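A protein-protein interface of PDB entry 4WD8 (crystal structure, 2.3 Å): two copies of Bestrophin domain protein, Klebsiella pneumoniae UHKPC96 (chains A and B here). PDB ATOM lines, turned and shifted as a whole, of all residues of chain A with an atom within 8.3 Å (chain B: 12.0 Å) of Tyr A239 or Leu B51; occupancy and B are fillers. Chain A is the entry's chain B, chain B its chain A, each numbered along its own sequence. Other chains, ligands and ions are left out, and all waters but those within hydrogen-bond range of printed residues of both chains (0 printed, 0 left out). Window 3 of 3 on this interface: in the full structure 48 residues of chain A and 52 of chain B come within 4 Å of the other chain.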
ATOM      1  N   SER A  38     -42.643   3.022  29.471  1.00  0.00           N
ATOM      2  CA  SER A  38     -41.305   2.599  29.061  1.00  0.00           C
ATOM      3  C   SER A  38     -41.207   1.090  28.842  1.00  0.00           C
ATOM      4  O   SER A  38     -40.577   0.631  27.888  1.00  0.00           O
ATOM      5  CB  SER A  38     -40.265   3.028  30.090  1.00  0.00           C
ATOM      6  OG  SER A  38     -40.087   4.431  30.097  1.00  0.00           O
ATOM      7  N   ILE A  39     -41.813   0.322  29.741  1.00  0.00           N
ATOM      8  CA  ILE A  39     -41.807  -1.129  29.622  1.00  0.00           C
ATOM      9  C   ILE A  39     -42.542  -1.563  28.355  1.00  0.00           C
ATOM     10  O   ILE A  39     -42.107  -2.479  27.658  1.00  0.00           O
ATOM     11  CB  ILE A  39     -42.410  -1.809  30.874  1.00  0.00           C
ATOM     12  CG1 ILE A  39     -41.664  -1.359  32.134  1.00  0.00           C
ATOM     13  CG2 ILE A  39     -42.381  -3.324  30.733  1.00  0.00           C
ATOM     14  CD1 ILE A  39     -42.258  -1.880  33.425  1.00  0.00           C
ATOM     15  N   ILE A  42     -40.254  -0.981  25.473  1.00  0.00           N
ATOM     16  CA  ILE A  42     -39.199  -1.990  25.424  1.00  0.00           C
ATOM     17  C   ILE A  42     -39.689  -3.291  24.802  1.00  0.00           C
ATOM     18  O   ILE A  42     -39.021  -3.863  23.942  1.00  0.00           O
ATOM     19  CB  ILE A  42     -38.588  -2.266  26.818  1.00  0.00           C
ATOM     20  CG1 ILE A  42     -37.728  -1.081  27.261  1.00  0.00           C
ATOM     21  CG2 ILE A  42     -37.726  -3.522  26.790  1.00  0.00           C
ATOM     22  CD1 ILE A  42     -37.020  -1.295  28.582  1.00  0.00           C
ATOM     23  N   ILE A  43     -40.862  -3.748  25.227  1.00  0.00           N
ATOM     24  CA  ILE A  43     -41.398  -5.013  24.745  1.00  0.00           C
ATOM     25  C   ILE A  43     -41.938  -4.926  23.315  1.00  0.00           C
ATOM     26  O   ILE A  43     -42.014  -5.936  22.613  1.00  0.00           O
ATOM     27  CB  ILE A  43     -42.485  -5.580  25.693  1.00  0.00           C
ATOM     28  CG1 ILE A  43     -43.696  -4.646  25.749  1.00  0.00           C
ATOM     29  CG2 ILE A  43     -41.920  -5.787  27.091  1.00  0.00           C
ATOM     30  CD1 ILE A  43     -44.853  -5.189  26.569  1.00  0.00           C
ATOM     31  N   GLN A  46     -39.476  -4.506  18.995  1.00  0.00           N
ATOM     32  CA  GLN A  46     -39.278  -5.487  17.930  1.00  0.00           C
ATOM     33  C   GLN A  46     -40.313  -5.299  16.828  1.00  0.00           C
ATOM     34  O   GLN A  46     -40.010  -5.412  15.643  1.00  0.00           O
ATOM     35  CB  GLN A  46     -39.360  -6.919  18.453  1.00  0.00           C
ATOM     36  CG  GLN A  46     -38.345  -7.283  19.513  1.00  0.00           C
ATOM     37  CD  GLN A  46     -38.509  -8.717  19.971  1.00  0.00           C
ATOM     38  OE1 GLN A  46     -38.175  -9.066  21.102  1.00  0.00           O
ATOM     39  NE2 GLN A  46     -39.018  -9.562  19.081  1.00  0.00           N
ATOM     40  N   LEU A 233     -37.252   6.875  22.623  1.00  0.00           N
ATOM     41  CA  LEU A 233     -35.932   6.655  23.212  1.00  0.00           C
ATOM     42  C   LEU A 233     -35.446   5.210  23.110  1.00  0.00           C
ATOM     43  O   LEU A 233     -34.240   4.966  23.053  1.00  0.00           O
ATOM     44  CB  LEU A 233     -35.918   7.084  24.686  1.00  0.00           C
ATOM     45  CG  LEU A 233     -36.086   8.564  25.051  1.00  0.00           C
ATOM     46  CD1 LEU A 233     -36.024   8.738  26.566  1.00  0.00           C
ATOM     47  CD2 LEU A 233     -35.051   9.444  24.362  1.00  0.00           C
ATOM     48  N   VAL A 234     -36.379   4.262  23.077  1.00  0.00           N
ATOM     49  CA  VAL A 234     -36.043   2.842  23.195  1.00  0.00           C
ATOM     50  C   VAL A 234     -35.038   2.351  22.142  1.00  0.00           C
ATOM     51  O   VAL A 234     -34.204   1.493  22.428  1.00  0.00           O
ATOM     52  CB  VAL A 234     -37.313   1.942  23.211  1.00  0.00           C
ATOM     53  CG1 VAL A 234     -38.000   1.938  21.853  1.00  0.00           C
ATOM     54  CG2 VAL A 234     -36.959   0.531  23.638  1.00  0.00           C
ATOM     55  N   GLY A 235     -35.100   2.911  20.938  1.00  0.00           N
ATOM     56  CA  GLY A 235     -34.193   2.526  19.873  1.00  0.00           C
ATOM     57  C   GLY A 235     -32.743   2.799  20.235  1.00  0.00           C
ATOM     58  O   GLY A 235     -31.837   2.090  19.789  1.00  0.00           O
ATOM     59  N   ASP A 236     -32.524   3.835  21.040  1.00  0.00           N
ATOM     60  CA  ASP A 236     -31.185   4.175  21.507  1.00  0.00           C
ATOM     61  C   ASP A 236     -30.849   3.516  22.844  1.00  0.00           C
ATOM     62  O   ASP A 236     -29.746   3.002  23.038  1.00  0.00           O
ATOM     63  CB  ASP A 236     -31.032   5.694  21.663  1.00  0.00           C
ATOM     64  CG  ASP A 236     -30.915   6.419  20.336  1.00  0.00           C
ATOM     65  OD1 ASP A 236     -31.050   5.770  19.278  1.00  0.00           O
ATOM     66  OD2 ASP A 236     -30.663   7.643  20.357  1.00  0.00           O
ATOM     67  N   LEU A 237     -31.809   3.537  23.761  1.00  0.00           N
ATOM     68  CA  LEU A 237     -31.550   3.188  25.154  1.00  0.00           C
ATOM     69  C   LEU A 237     -31.852   1.740  25.498  1.00  0.00           C
ATOM     70  O   LEU A 237     -31.265   1.186  26.429  1.00  0.00           O
ATOM     71  CB  LEU A 237     -32.323   4.128  26.083  1.00  0.00           C
ATOM     72  CG  LEU A 237     -32.018   5.615  25.885  1.00  0.00           C
ATOM     73  CD1 LEU A 237     -32.747   6.450  26.917  1.00  0.00           C
ATOM     74  CD2 LEU A 237     -30.517   5.869  25.946  1.00  0.00           C
ATOM     75  N   HIS A 238     -32.763   1.132  24.743  1.00  0.00           N
ATOM     76  CA  HIS A 238     -33.164  -0.252  24.982  1.00  0.00           C
ATOM     77  C   HIS A 238     -33.629  -0.453  26.433  1.00  0.00           C
ATOM     78  O   HIS A 238     -34.607   0.159  26.855  1.00  0.00           O
ATOM     79  CB  HIS A 238     -32.031  -1.211  24.593  1.00  0.00           C
ATOM     80  CG  HIS A 238     -31.598  -1.078  23.163  1.00  0.00           C
ATOM     81  ND1 HIS A 238     -32.316  -1.613  22.112  1.00  0.00           N
ATOM     82  CD2 HIS A 238     -30.540  -0.442  22.605  1.00  0.00           C
ATOM     83  CE1 HIS A 238     -31.706  -1.331  20.974  1.00  0.00           C
ATOM     84  NE2 HIS A 238     -30.627  -0.620  21.245  1.00  0.00           N
ATOM     85  N   TYR A 239     -32.924  -1.286  27.195  1.00  0.00           N
ATOM     86  CA  TYR A 239     -33.318  -1.574  28.579  1.00  0.00           C
ATOM     87  C   TYR A 239     -33.202  -0.389  29.548  1.00  0.00           C
ATOM     88  O   TYR A 239     -33.865  -0.361  30.586  1.00  0.00           O
ATOM     89  CB  TYR A 239     -32.530  -2.767  29.122  1.00  0.00           C
ATOM     90  CG  TYR A 239     -33.051  -4.099  28.633  1.00  0.00           C
ATOM     91  CD1 TYR A 239     -34.409  -4.291  28.412  1.00  0.00           C
ATOM     92  CD2 TYR A 239     -32.193  -5.165  28.405  1.00  0.00           C
ATOM     93  CE1 TYR A 239     -34.895  -5.501  27.970  1.00  0.00           C
ATOM     94  CE2 TYR A 239     -32.671  -6.385  27.965  1.00  0.00           C
ATOM     95  CZ  TYR A 239     -34.023  -6.546  27.748  1.00  0.00           C
ATOM     96  OH  TYR A 239     -34.507  -7.753  27.307  1.00  0.00           O
ATOM     97  N   MET A 240     -32.361   0.582  29.216  1.00  0.00           N
ATOM     98  CA  MET A 240     -32.186   1.755  30.068  1.00  0.00           C
ATOM     99  C   MET A 240     -33.312   2.775  29.899  1.00  0.00           C
ATOM    100  O   MET A 240     -33.293   3.837  30.521  1.00  0.00           O
ATOM    101  CB  MET A 240     -30.832   2.414  29.804  1.00  0.00           C
ATOM    102  CG  MET A 240     -29.659   1.680  30.435  1.00  0.00           C
ATOM    103  SD  MET A 240     -29.676   1.737  32.243  1.00  0.00           S
ATOM    104  CE  MET A 240     -29.717   3.503  32.536  1.00  0.00           C
ATOM    105  N   THR A 241     -34.290   2.441  29.059  1.00  0.00           N
ATOM    106  CA  THR A 241     -35.410   3.335  28.753  1.00  0.00           C
ATOM    107  C   THR A 241     -36.208   3.860  29.961  1.00  0.00           C
ATOM    108  O   THR A 241     -36.419   5.068  30.064  1.00  0.00           O
ATOM    109  CB  THR A 241     -36.361   2.710  27.696  1.00  0.00           C
ATOM    110  OG1 THR A 241     -35.642   2.519  26.473  1.00  0.00           O
ATOM    111  CG2 THR A 241     -37.555   3.612  27.427  1.00  0.00           C
ATOM    112  N   PRO A 242     -36.652   2.972  30.875  1.00  0.00           N
ATOM    113  CA  PRO A 242     -37.463   3.493  31.989  1.00  0.00           C
ATOM    114  C   PRO A 242     -36.735   4.477  32.905  1.00  0.00           C
ATOM    115  O   PRO A 242     -37.354   5.415  33.404  1.00  0.00           O
ATOM    116  CB  PRO A 242     -37.854   2.224  32.760  1.00  0.00           C
ATOM    117  CG  PRO A 242     -36.833   1.211  32.377  1.00  0.00           C
ATOM    118  CD  PRO A 242     -36.521   1.506  30.945  1.00  0.00           C
ATOM    119  N   PHE A 243     -35.439   4.265  33.108  1.00  0.00           N
ATOM    120  CA  PHE A 243     -34.643   5.113  33.989  1.00  0.00           C
ATOM    121  C   PHE A 243     -34.480   6.524  33.436  1.00  0.00           C
ATOM    122  O   PHE A 243     -34.709   7.509  34.139  1.00  0.00           O
ATOM    123  CB  PHE A 243     -33.268   4.487  34.219  1.00  0.00           C
ATOM    124  CG  PHE A 243     -33.323   3.117  34.829  1.00  0.00           C
ATOM    125  CD1 PHE A 243     -33.725   2.939  36.144  1.00  0.00           C
ATOM    126  CD2 PHE A 243     -32.987   2.001  34.076  1.00  0.00           C
ATOM    127  CE1 PHE A 243     -33.778   1.672  36.700  1.00  0.00           C
ATOM    128  CE2 PHE A 243     -33.039   0.732  34.626  1.00  0.00           C
ATOM    129  CZ  PHE A 243     -33.435   0.568  35.939  1.00  0.00           C
ATOM    130  N   VAL A 244     -34.079   6.615  32.173  1.00  0.00           N
ATOM    131  CA  VAL A 244     -33.858   7.904  31.527  1.00  0.00           C
ATOM    132  C   VAL A 244     -35.171   8.640  31.261  1.00  0.00           C
ATOM    133  O   VAL A 244     -35.234   9.865  31.359  1.00  0.00           O
ATOM    134  CB  VAL A 244     -33.057   7.744  30.220  1.00  0.00           C
ATOM    135  CG1 VAL A 244     -32.886   9.085  29.511  1.00  0.00           C
ATOM    136  CG2 VAL A 244     -31.703   7.121  30.511  1.00  0.00           C
ATOM    137  N   ILE B  43     -14.472   0.466  32.549  1.00  0.00           N
ATOM    138  CA  ILE B  43     -14.217  -0.956  32.787  1.00  0.00           C
ATOM    139  C   ILE B  43     -15.471  -1.837  32.719  1.00  0.00           C
ATOM    140  O   ILE B  43     -15.375  -3.037  32.459  1.00  0.00           O
ATOM    141  CB  ILE B  43     -13.477  -1.195  34.129  1.00  0.00           C
ATOM    142  CG1 ILE B  43     -14.340  -0.748  35.310  1.00  0.00           C
ATOM    143  CG2 ILE B  43     -12.147  -0.457  34.145  1.00  0.00           C
ATOM    144  CD1 ILE B  43     -13.728  -1.050  36.664  1.00  0.00           C
ATOM    145  N   SER B  44     -16.640  -1.240  32.937  1.00  0.00           N
ATOM    146  CA  SER B  44     -17.893  -1.997  32.943  1.00  0.00           C
ATOM    147  C   SER B  44     -18.605  -1.903  31.599  1.00  0.00           C
ATOM    148  O   SER B  44     -19.636  -2.544  31.384  1.00  0.00           O
ATOM    149  CB  SER B  44     -18.821  -1.533  34.067  1.00  0.00           C
ATOM    150  OG  SER B  44     -19.259  -0.207  33.843  1.00  0.00           O
ATOM    151  N   TYR B  45     -18.050  -1.094  30.704  1.00  0.00           N
ATOM    152  CA  TYR B  45     -18.593  -0.925  29.360  1.00  0.00           C
ATOM    153  C   TYR B  45     -18.653  -2.255  28.600  1.00  0.00           C
ATOM    154  O   TYR B  45     -19.431  -2.407  27.658  1.00  0.00           O
ATOM    155  CB  TYR B  45     -17.789   0.125  28.579  1.00  0.00           C
ATOM    156  CG  TYR B  45     -18.253   0.333  27.156  1.00  0.00           C
ATOM    157  CD1 TYR B  45     -19.496   0.888  26.882  1.00  0.00           C
ATOM    158  CD2 TYR B  45     -17.443  -0.029  26.083  1.00  0.00           C
ATOM    159  CE1 TYR B  45     -19.922   1.075  25.579  1.00  0.00           C
ATOM    160  CE2 TYR B  45     -17.858   0.153  24.780  1.00  0.00           C
ATOM    161  CZ  TYR B  45     -19.098   0.705  24.530  1.00  0.00           C
ATOM    162  OH  TYR B  45     -19.513   0.888  23.227  1.00  0.00           O
ATOM    163  N   GLN B  46     -17.827  -3.213  29.014  1.00  0.00           N
ATOM    164  CA  GLN B  46     -17.843  -4.549  28.429  1.00  0.00           C
ATOM    165  C   GLN B  46     -19.199  -5.233  28.596  1.00  0.00           C
ATOM    166  O   GLN B  46     -19.741  -5.792  27.643  1.00  0.00           O
ATOM    167  CB  GLN B  46     -16.772  -5.429  29.077  1.00  0.00           C
ATOM    168  CG  GLN B  46     -15.346  -4.922  28.949  1.00  0.00           C
ATOM    169  CD  GLN B  46     -14.354  -5.830  29.653  1.00  0.00           C
ATOM    170  OE1 GLN B  46     -14.379  -5.962  30.877  1.00  0.00           O
ATOM    171  NE2 GLN B  46     -13.487  -6.476  28.880  1.00  0.00           N
ATOM    172  N   TRP B  47     -19.754  -5.164  29.802  1.00  0.00           N
ATOM    173  CA  TRP B  47     -20.966  -5.911  30.132  1.00  0.00           C
ATOM    174  C   TRP B  47     -22.230  -5.172  29.696  1.00  0.00           C
ATOM    175  O   TRP B  47     -23.342  -5.589  30.021  1.00  0.00           O
ATOM    176  CB  TRP B  47     -21.033  -6.196  31.636  1.00  0.00           C
ATOM    177  CG  TRP B  47     -19.751  -6.704  32.234  1.00  0.00           C
ATOM    178  CD1 TRP B  47     -18.881  -6.002  33.018  1.00  0.00           C
ATOM    179  CD2 TRP B  47     -19.205  -8.026  32.114  1.00  0.00           C
ATOM    180  NE1 TRP B  47     -17.825  -6.800  33.386  1.00  0.00           N
ATOM    181  CE2 TRP B  47     -17.999  -8.046  32.845  1.00  0.00           C
ATOM    182  CE3 TRP B  47     -19.616  -9.189  31.457  1.00  0.00           C
ATOM    183  CZ2 TRP B  47     -17.201  -9.186  32.936  1.00  0.00           C
ATOM    184  CZ3 TRP B  47     -18.820 -10.322  31.550  1.00  0.00           C
ATOM    185  CH2 TRP B  47     -17.626 -10.311  32.284  1.00  0.00           C
ATOM    186  N   TYR B  48     -22.050  -4.074  28.971  1.00  0.00           N
ATOM    187  CA  TYR B  48     -23.166  -3.259  28.498  1.00  0.00           C
ATOM    188  C   TYR B  48     -24.097  -4.038  27.572  1.00  0.00           C
ATOM    189  O   TYR B  48     -25.311  -4.065  27.775  1.00  0.00           O
ATOM    190  CB  TYR B  48     -22.640  -2.020  27.776  1.00  0.00           C
ATOM    191  CG  TYR B  48     -22.576  -0.772  28.626  1.00  0.00           C
ATOM    192  CD1 TYR B  48     -22.093  -0.814  29.930  1.00  0.00           C
ATOM    193  CD2 TYR B  48     -22.975   0.456  28.112  1.00  0.00           C
ATOM    194  CE1 TYR B  48     -22.027   0.331  30.701  1.00  0.00           C
ATOM    195  CE2 TYR B  48     -22.911   1.604  28.873  1.00  0.00           C
ATOM    196  CZ  TYR B  48     -22.437   1.536  30.164  1.00  0.00           C
ATOM    197  OH  TYR B  48     -22.375   2.686  30.912  1.00  0.00           O
ATOM    198  N   GLU B  49     -23.509  -4.654  26.548  1.00  0.00           N
ATOM    199  CA  GLU B  49     -24.248  -5.455  25.575  1.00  0.00           C
ATOM    200  C   GLU B  49     -24.820  -6.728  26.196  1.00  0.00           C
ATOM    201  O   GLU B  49     -25.935  -7.143  25.876  1.00  0.00           O
ATOM    202  CB  GLU B  49     -23.355  -5.808  24.381  1.00  0.00           C
ATOM    203  N   GLN B  50     -24.046  -7.350  27.083  1.00  0.00           N
ATOM    204  CA  GLN B  50     -24.450  -8.604  27.716  1.00  0.00           C
ATOM    205  C   GLN B  50     -25.608  -8.419  28.697  1.00  0.00           C
ATOM    206  O   GLN B  50     -26.071  -9.379  29.309  1.00  0.00           O
ATOM    207  CB  GLN B  50     -23.257  -9.259  28.419  1.00  0.00           C
ATOM    208  N   LEU B  51     -26.070  -7.182  28.842  1.00  0.00           N
ATOM    209  CA  LEU B  51     -27.212  -6.891  29.695  1.00  0.00           C
ATOM    210  C   LEU B  51     -28.323  -6.242  28.879  1.00  0.00           C
ATOM    211  O   LEU B  51     -29.498  -6.325  29.234  1.00  0.00           O
ATOM    212  CB  LEU B  51     -26.801  -5.982  30.858  1.00  0.00           C
ATOM    213  N   GLY B  52     -27.939  -5.600  27.779  1.00  0.00           N
ATOM    214  CA  GLY B  52     -28.887  -4.949  26.894  1.00  0.00           C
ATOM    215  C   GLY B  52     -29.040  -3.478  27.231  1.00  0.00           C
ATOM    216  O   GLY B  52     -30.004  -2.832  26.822  1.00  0.00           O
ATOM    217  N   ILE B  53     -28.084  -2.947  27.988  1.00  0.00           N
ATOM    218  CA  ILE B  53     -28.121  -1.542  28.377  1.00  0.00           C
ATOM    219  C   ILE B  53     -27.254  -0.647  27.483  1.00  0.00           C
ATOM    220  O   ILE B  53     -26.055  -0.879  27.312  1.00  0.00           O
ATOM    221  CB  ILE B  53     -27.764  -1.357  29.874  1.00  0.00           C
ATOM    222  CG1 ILE B  53     -26.350  -1.867  30.163  1.00  0.00           C
ATOM    223  CG2 ILE B  53     -28.756  -2.108  30.745  1.00  0.00           C
ATOM    224  CD1 ILE B  53     -25.951  -1.787  31.619  1.00  0.00           C
ATOM    225  N   HIS B  54     -27.892   0.356  26.889  1.00  0.00           N
ATOM    226  CA  HIS B  54     -27.207   1.374  26.101  1.00  0.00           C
ATOM    227  C   HIS B  54     -27.561   2.778  26.569  1.00  0.00           C
ATOM    228  O   HIS B  54     -28.689   3.048  26.980  1.00  0.00           O
ATOM    229  CB  HIS B  54     -27.521   1.230  24.611  1.00  0.00           C
ATOM    230  CG  HIS B  54     -26.913   0.015  23.984  1.00  0.00           C
ATOM    231  ND1 HIS B  54     -27.186  -1.268  24.413  1.00  0.00           N
ATOM    232  CD2 HIS B  54     -26.017  -0.110  22.978  1.00  0.00           C
ATOM    233  CE1 HIS B  54     -26.497  -2.129  23.685  1.00  0.00           C
ATOM    234  NE2 HIS B  54     -25.779  -1.451  22.808  1.00  0.00           N
ATOM    235  N   LEU B  55     -26.579   3.668  26.518  1.00  0.00           N
ATOM    236  CA  LEU B  55     -26.792   5.059  26.880  1.00  0.00           C
ATOM    237  C   LEU B  55     -26.124   5.956  25.847  1.00  0.00           C
ATOM    238  O   LEU B  55     -24.900   5.957  25.703  1.00  0.00           O
ATOM    239  CB  LEU B  55     -26.254   5.346  28.284  1.00  0.00           C
ATOM    240  CG  LEU B  55     -27.035   4.711  29.438  1.00  0.00           C
ATOM    241  CD1 LEU B  55     -26.300   4.890  30.755  1.00  0.00           C
ATOM    242  CD2 LEU B  55     -28.441   5.289  29.525  1.00  0.00           C
ATOM    243  N   THR B  56     -26.949   6.678  25.094  1.00  0.00           N
ATOM    244  CA  THR B  56     -26.455   7.598  24.076  1.00  0.00           C
ATOM    245  C   THR B  56     -26.453   9.037  24.584  1.00  0.00           C
ATOM    246  O   THR B  56     -27.050   9.348  25.615  1.00  0.00           O
ATOM    247  CB  THR B  56     -27.283   7.509  22.776  1.00  0.00           C
ATOM    248  OG1 THR B  56     -28.666   7.746  23.068  1.00  0.00           O
ATOM    249  CG2 THR B  56     -27.126   6.131  22.132  1.00  0.00           C
ATOM    250  N   PRO B  59     -30.269  11.819  24.390  1.00  0.00           N
ATOM    251  CA  PRO B  59     -31.253  12.041  25.457  1.00  0.00           C
ATOM    252  C   PRO B  59     -30.690  12.878  26.602  1.00  0.00           C
ATOM    253  O   PRO B  59     -31.433  13.625  27.240  1.00  0.00           O
ATOM    254  CB  PRO B  59     -31.566  10.622  25.946  1.00  0.00           C
ATOM    255  CG  PRO B  59     -31.224   9.743  24.798  1.00  0.00           C
ATOM    256  CD  PRO B  59     -30.027  10.380  24.174  1.00  0.00           C
ATOM    257  N   PHE B  60     -29.393  12.747  26.861  1.00  0.00           N
ATOM    258  CA  PHE B  60     -28.745  13.526  27.913  1.00  0.00           C
ATOM    259  C   PHE B  60     -28.485  14.971  27.484  1.00  0.00           C
ATOM    260  O   PHE B  60     -28.313  15.857  28.323  1.00  0.00           O
ATOM    261  CB  PHE B  60     -27.463  12.847  28.397  1.00  0.00           C
ATOM    262  CG  PHE B  60     -27.707  11.757  29.398  1.00  0.00           C
ATOM    263  CD1 PHE B  60     -28.155  10.513  28.991  1.00  0.00           C
ATOM    264  CD2 PHE B  60     -27.503  11.983  30.747  1.00  0.00           C
ATOM    265  CE1 PHE B  60     -28.388   9.511  29.912  1.00  0.00           C
ATOM    266  CE2 PHE B  60     -27.736  10.990  31.672  1.00  0.00           C
ATOM    267  CZ  PHE B  60     -28.180   9.753  31.257  1.00  0.00           C
ATOM    268  N   LEU B 228     -24.726  10.108  36.190  1.00  0.00           N
ATOM    269  CA  LEU B 228     -25.158   9.269  35.077  1.00  0.00           C
ATOM    270  C   LEU B 228     -24.417   9.608  33.787  1.00  0.00           C
ATOM    271  O   LEU B 228     -24.297   8.771  32.895  1.00  0.00           O
ATOM    272  CB  LEU B 228     -26.664   9.421  34.856  1.00  0.00           C
ATOM    273  CG  LEU B 228     -27.555   8.275  35.325  1.00  0.00           C
ATOM    274  CD1 LEU B 228     -27.144   7.795  36.708  1.00  0.00           C
ATOM    275  CD2 LEU B 228     -29.004   8.724  35.325  1.00  0.00           C
ATOM    276  N   PHE B 231     -21.572   7.365  32.068  1.00  0.00           N
ATOM    277  CA  PHE B 231     -22.140   6.157  31.483  1.00  0.00           C
ATOM    278  C   PHE B 231     -22.745   6.432  30.112  1.00  0.00           C
ATOM    279  O   PHE B 231     -22.830   5.538  29.272  1.00  0.00           O
ATOM    280  CB  PHE B 231     -23.189   5.548  32.414  1.00  0.00           C
ATOM    281  CG  PHE B 231     -22.617   4.998  33.687  1.00  0.00           C
ATOM    282  CD1 PHE B 231     -22.398   5.822  34.776  1.00  0.00           C
ATOM    283  CD2 PHE B 231     -22.289   3.655  33.792  1.00  0.00           C
ATOM    284  CE1 PHE B 231     -21.866   5.318  35.947  1.00  0.00           C
ATOM    285  CE2 PHE B 231     -21.758   3.143  34.961  1.00  0.00           C
ATOM    286  CZ  PHE B 231     -21.547   3.978  36.041  1.00  0.00           C
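The side-chain carboxylate (OD2) of Asp A236 sits at hydrogen-bond distance from the side-chain hydroxyl (OG1) of Thr B56 (3.4 Å).
N of Tyr A239 sits at hydrogen-bond distance from O of Gly B52.
O of Leu A237 lies close to O of His B54, 3.2 Å away.
O of Gly A235 is in hydrogen-bond range of NE2 of His A238 (3.3 Å).
N of Ile B53 sits at hydrogen-bond distance from O of Tyr B48.
The backbone carbonyl oxygen (O) of His A238 sits at hydrogen-bond distance from the side-chain hydroxyl (OG1) of Thr A241, at 2.6 Å.
Leu A233 touches Pro B59 (CD2 to CG, 3.9 Å).
Asp A236 touches His B54 (O to CB, 3.3 Å).
Leu B55 touches Leu A237 (CA to CD2, 3.9 Å).
Thr B56 touches Leu A237.
Gly B52 touches His A238.
CD2 of His A238 touches ND1 of His B54, at 3.9 Å.
Tyr A239 touches Leu B51 (CD2 to O, 3.0 Å).
Ile B53 touches Met A240 (CB to CG, 3.6 Å).
O of His B54 touches CB of Met A240 (3.6 Å).
Met A240 touches Leu B55 (CE to CD2, 3.7 Å).
Ile A42 touches none of the printed residues of chain B.
His A238 touches two residues of chain B.
Of chain B, only Leu B51 (3.0 Å) and Gly B52 (3.3 Å) come within 4 Å of Tyr A239.
No residue of chain B comes within 4 Å of Thr A241.
No residue of chain B comes within 4 Å of Pro A242.
Printed residues of chain B within 4 Å of Val A244: Leu B55.
Glu B49 touches none of the printed residues of chain A.
Leu B51 touches just one residue of chain A: Tyr A239.
Gly B52 touches two residues of chain A.
Printed residues of chain A within 4 Å of Ile B53: Met A240.
Of the printed residues of chain A, His B54 touches Asp A236 (3.3 Å), Leu A237 (3.2 Å), His A238 (3.9 Å) and Met A240 (3.6 Å).
Of the 18 printed residues of chain B, 7 touch a printed residue of chain A.
Printed residues of chain B that touch a printed residue of chain A: Leu B51, Gly B52, Ile B53, His B54, Leu B55, Thr B56 and Pro B59.
Hydrophobic or aromatic side chains of chain B within 4 Å of the printed part of chain A: Ile B53, His B54, Leu B55 and Pro B59.
Of the 17 printed residues of chain A, 7 touch a printed residue of chain B.
Hydrophobic or aromatic side chains of chain A that line the printed part of chain B: Leu A233, Leu A237, His A238, Tyr A239, Met A240 and Val A244.
Along chain A the printed residues that touch a printed residue of chain B span positions 233 to 244.
2 positions are printed for both chains.
Of the 14 pairs that touch across the chains among the printed residues, none has its exchanged pair printed and touching as well.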
